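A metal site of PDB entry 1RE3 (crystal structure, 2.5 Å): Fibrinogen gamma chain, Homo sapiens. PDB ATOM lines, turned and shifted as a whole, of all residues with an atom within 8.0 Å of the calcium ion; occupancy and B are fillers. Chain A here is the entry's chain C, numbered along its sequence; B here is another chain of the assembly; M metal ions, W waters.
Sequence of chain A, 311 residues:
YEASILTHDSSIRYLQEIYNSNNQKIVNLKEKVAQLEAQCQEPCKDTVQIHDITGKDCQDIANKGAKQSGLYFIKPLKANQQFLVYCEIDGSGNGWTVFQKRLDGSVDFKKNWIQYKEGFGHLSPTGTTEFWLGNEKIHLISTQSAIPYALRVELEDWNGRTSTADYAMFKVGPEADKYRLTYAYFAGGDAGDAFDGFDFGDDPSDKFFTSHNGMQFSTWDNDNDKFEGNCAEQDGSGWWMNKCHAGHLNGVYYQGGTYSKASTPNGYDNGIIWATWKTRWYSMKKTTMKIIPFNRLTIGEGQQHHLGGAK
Asp 202 touches the calcium ion (O to CA, 3.9 Å). CA of Pro 204 touches the calcium ion, at 3.9 Å. Along chain A the residues within 4 Å of the calcium ion span positions 199 to 206.
The calcium ion is bound by O of Asp 203 (2.2 Å), OD1 of Asp 199 (2.3 Å), O of Gly 201 (2.5 Å), water W1 (2.6 Å) and OD2 of Asp 206 (2.9 Å). The calcium ion has five donor atoms within binding distance.
NE2 of His 2 of chain B lies within hydrogen-bond range of OD2 of Asp 203 (3.4 Å). The side-chain carboxylate (OD1) of Asp 203 sits at hydrogen-bond distance from the side-chain hydroxyl (OG) of Ser 205 (2.7 Å).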
ATOM      1  N   PHE A 198       8.936   3.964 -15.655  1.00  0.00           N
ATOM      2  CA  PHE A 198       8.295   2.660 -15.797  1.00  0.00           C
ATOM      3  C   PHE A 198       9.204   1.580 -16.392  1.00  0.00           C
ATOM      4  O   PHE A 198       9.999   1.839 -17.309  1.00  0.00           O
ATOM      5  CB  PHE A 198       7.041   2.782 -16.667  1.00  0.00           C
ATOM      6  CG  PHE A 198       6.134   1.603 -16.562  1.00  0.00           C
ATOM      7  CD1 PHE A 198       5.231   1.488 -15.508  1.00  0.00           C
ATOM      8  CD2 PHE A 198       6.220   0.563 -17.477  1.00  0.00           C
ATOM      9  CE1 PHE A 198       4.424   0.355 -15.372  1.00  0.00           C
ATOM     10  CE2 PHE A 198       5.424  -0.572 -17.351  1.00  0.00           C
ATOM     11  CZ  PHE A 198       4.519  -0.681 -16.290  1.00  0.00           C
ATOM     12  N   ASP A 199       9.078   0.365 -15.861  1.00  0.00           N
ATOM     13  CA  ASP A 199       9.849  -0.795 -16.308  1.00  0.00           C
ATOM     14  C   ASP A 199       9.116  -1.431 -17.506  1.00  0.00           C
ATOM     15  O   ASP A 199       8.444  -2.448 -17.379  1.00  0.00           O
ATOM     16  CB  ASP A 199       9.961  -1.798 -15.150  1.00  0.00           C
ATOM     17  CG  ASP A 199      10.920  -2.939 -15.436  1.00  0.00           C
ATOM     18  OD1 ASP A 199      11.498  -3.011 -16.545  1.00  0.00           O
ATOM     19  OD2 ASP A 199      11.098  -3.784 -14.532  1.00  0.00           O
ATOM     20  N   PHE A 200       9.256  -0.794 -18.668  1.00  0.00           N
ATOM     21  CA  PHE A 200       8.617  -1.245 -19.887  1.00  0.00           C
ATOM     22  C   PHE A 200       9.066  -2.615 -20.382  1.00  0.00           C
ATOM     23  O   PHE A 200       8.250  -3.411 -20.850  1.00  0.00           O
ATOM     24  CB  PHE A 200       8.848  -0.227 -21.000  1.00  0.00           C
ATOM     25  CG  PHE A 200       8.143   1.081 -20.786  1.00  0.00           C
ATOM     26  CD1 PHE A 200       6.754   1.162 -20.879  1.00  0.00           C
ATOM     27  CD2 PHE A 200       8.867   2.241 -20.496  1.00  0.00           C
ATOM     28  CE1 PHE A 200       6.099   2.369 -20.676  1.00  0.00           C
ATOM     29  CE2 PHE A 200       8.219   3.459 -20.289  1.00  0.00           C
ATOM     30  CZ  PHE A 200       6.829   3.524 -20.381  1.00  0.00           C
ATOM     31  N   GLY A 201      10.363  -2.894 -20.283  1.00  0.00           N
ATOM     32  CA  GLY A 201      10.845  -4.179 -20.752  1.00  0.00           C
ATOM     33  C   GLY A 201      12.204  -4.626 -20.250  1.00  0.00           C
ATOM     34  O   GLY A 201      12.633  -4.281 -19.148  1.00  0.00           O
ATOM     35  N   ASP A 202      12.871  -5.408 -21.100  1.00  0.00           N
ATOM     36  CA  ASP A 202      14.179  -5.989 -20.823  1.00  0.00           C
ATOM     37  C   ASP A 202      15.283  -5.054 -20.318  1.00  0.00           C
ATOM     38  O   ASP A 202      15.938  -5.346 -19.326  1.00  0.00           O
ATOM     39  CB  ASP A 202      14.670  -6.733 -22.065  1.00  0.00           C
ATOM     40  CG  ASP A 202      15.787  -7.689 -21.767  1.00  0.00           C
ATOM     41  OD1 ASP A 202      15.631  -8.512 -20.846  1.00  0.00           O
ATOM     42  OD2 ASP A 202      16.827  -7.637 -22.454  1.00  0.00           O
ATOM     43  N   ASP A 203      15.495  -3.935 -21.017  1.00  0.00           N
ATOM     44  CA  ASP A 203      16.530  -2.980 -20.633  1.00  0.00           C
ATOM     45  C   ASP A 203      16.425  -2.695 -19.136  1.00  0.00           C
ATOM     46  O   ASP A 203      15.351  -2.367 -18.644  1.00  0.00           O
ATOM     47  CB  ASP A 203      16.385  -1.679 -21.428  1.00  0.00           C
ATOM     48  CG  ASP A 203      17.673  -0.880 -21.477  1.00  0.00           C
ATOM     49  OD1 ASP A 203      18.276  -0.636 -20.406  1.00  0.00           O
ATOM     50  OD2 ASP A 203      18.081  -0.481 -22.591  1.00  0.00           O
ATOM     51  N   PRO A 204      17.544  -2.829 -18.397  1.00  0.00           N
ATOM     52  CA  PRO A 204      17.538  -2.582 -16.956  1.00  0.00           C
ATOM     53  C   PRO A 204      17.594  -1.099 -16.563  1.00  0.00           C
ATOM     54  O   PRO A 204      17.353  -0.761 -15.411  1.00  0.00           O
ATOM     55  CB  PRO A 204      18.768  -3.345 -16.472  1.00  0.00           C
ATOM     56  CG  PRO A 204      19.725  -3.155 -17.607  1.00  0.00           C
ATOM     57  CD  PRO A 204      18.840  -3.387 -18.829  1.00  0.00           C
ATOM     58  N   SER A 205      17.914  -0.236 -17.530  1.00  0.00           N
ATOM     59  CA  SER A 205      17.980   1.193 -17.249  1.00  0.00           C
ATOM     60  C   SER A 205      16.672   1.851 -17.710  1.00  0.00           C
ATOM     61  O   SER A 205      16.584   3.067 -17.882  1.00  0.00           O
ATOM     62  CB  SER A 205      19.183   1.799 -17.967  1.00  0.00           C
ATOM     63  OG  SER A 205      19.010   1.759 -19.363  1.00  0.00           O
ATOM     64  N   ASP A 206      15.670   1.001 -17.900  1.00  0.00           N
ATOM     65  CA  ASP A 206      14.310   1.359 -18.327  1.00  0.00           C
ATOM     66  C   ASP A 206      13.628   2.462 -17.500  1.00  0.00           C
ATOM     67  O   ASP A 206      13.394   3.577 -17.968  1.00  0.00           O
ATOM     68  CB  ASP A 206      13.428   0.110 -18.264  1.00  0.00           C
ATOM     69  CG  ASP A 206      12.959  -0.337 -19.617  1.00  0.00           C
ATOM     70  OD1 ASP A 206      12.793   0.543 -20.495  1.00  0.00           O
ATOM     71  OD2 ASP A 206      12.751  -1.544 -19.819  1.00  0.00           O
ATOM     72  N   LYS A 207      13.266   2.080 -16.274  1.00  0.00           N
ATOM     73  CA  LYS A 207      12.580   2.918 -15.303  1.00  0.00           C
ATOM     74  C   LYS A 207      13.365   4.198 -15.025  1.00  0.00           C
ATOM     75  O   LYS A 207      12.784   5.281 -14.877  1.00  0.00           O
ATOM     76  CB  LYS A 207      12.410   2.106 -13.997  1.00  0.00           C
ATOM     77  CG  LYS A 207      11.257   2.471 -13.088  1.00  0.00           C
ATOM     78  CD  LYS A 207      11.247   1.521 -11.890  1.00  0.00           C
ATOM     79  CE  LYS A 207       9.990   1.636 -11.037  1.00  0.00           C
ATOM     80  NZ  LYS A 207       9.855   2.943 -10.370  1.00  0.00           N
ATOM     81  N   PHE A 208      14.682   4.060 -14.963  1.00  0.00           N
ATOM     82  CA  PHE A 208      15.574   5.186 -14.681  1.00  0.00           C
ATOM     83  C   PHE A 208      15.465   6.302 -15.697  1.00  0.00           C
ATOM     84  O   PHE A 208      15.317   7.472 -15.338  1.00  0.00           O
ATOM     85  CB  PHE A 208      17.034   4.708 -14.624  1.00  0.00           C
ATOM     86  CG  PHE A 208      18.025   5.803 -14.340  1.00  0.00           C
ATOM     87  CD1 PHE A 208      18.149   6.333 -13.063  1.00  0.00           C
ATOM     88  CD2 PHE A 208      18.853   6.298 -15.358  1.00  0.00           C
ATOM     89  CE1 PHE A 208      19.094   7.335 -12.787  1.00  0.00           C
ATOM     90  CE2 PHE A 208      19.795   7.300 -15.095  1.00  0.00           C
ATOM     91  CZ  PHE A 208      19.913   7.825 -13.802  1.00  0.00           C
ATOM     92  N   HIS B   2      10.677   4.639 -23.513  1.00  0.00           N
ATOM     93  CA  HIS B   2      12.120   4.530 -23.361  1.00  0.00           C
ATOM     94  C   HIS B   2      12.795   4.519 -24.717  1.00  0.00           C
ATOM     95  O   HIS B   2      12.259   4.002 -25.692  1.00  0.00           O
ATOM     96  CB  HIS B   2      12.478   3.244 -22.609  1.00  0.00           C
ATOM     97  CG  HIS B   2      13.945   3.001 -22.499  1.00  0.00           C
ATOM     98  ND1 HIS B   2      14.829   3.919 -21.977  1.00  0.00           N
ATOM     99  CD2 HIS B   2      14.695   1.910 -22.809  1.00  0.00           C
ATOM    100  CE1 HIS B   2      16.047   3.413 -21.963  1.00  0.00           C
ATOM    101  NE2 HIS B   2      15.994   2.191 -22.471  1.00  0.00           N
HETATM  102 CA    CA M   1      13.650  -2.825 -17.382  1.00  0.00          CA
HETATM  103  O   HOH W   1      14.234  -2.004 -14.953  1.00  0.00           O
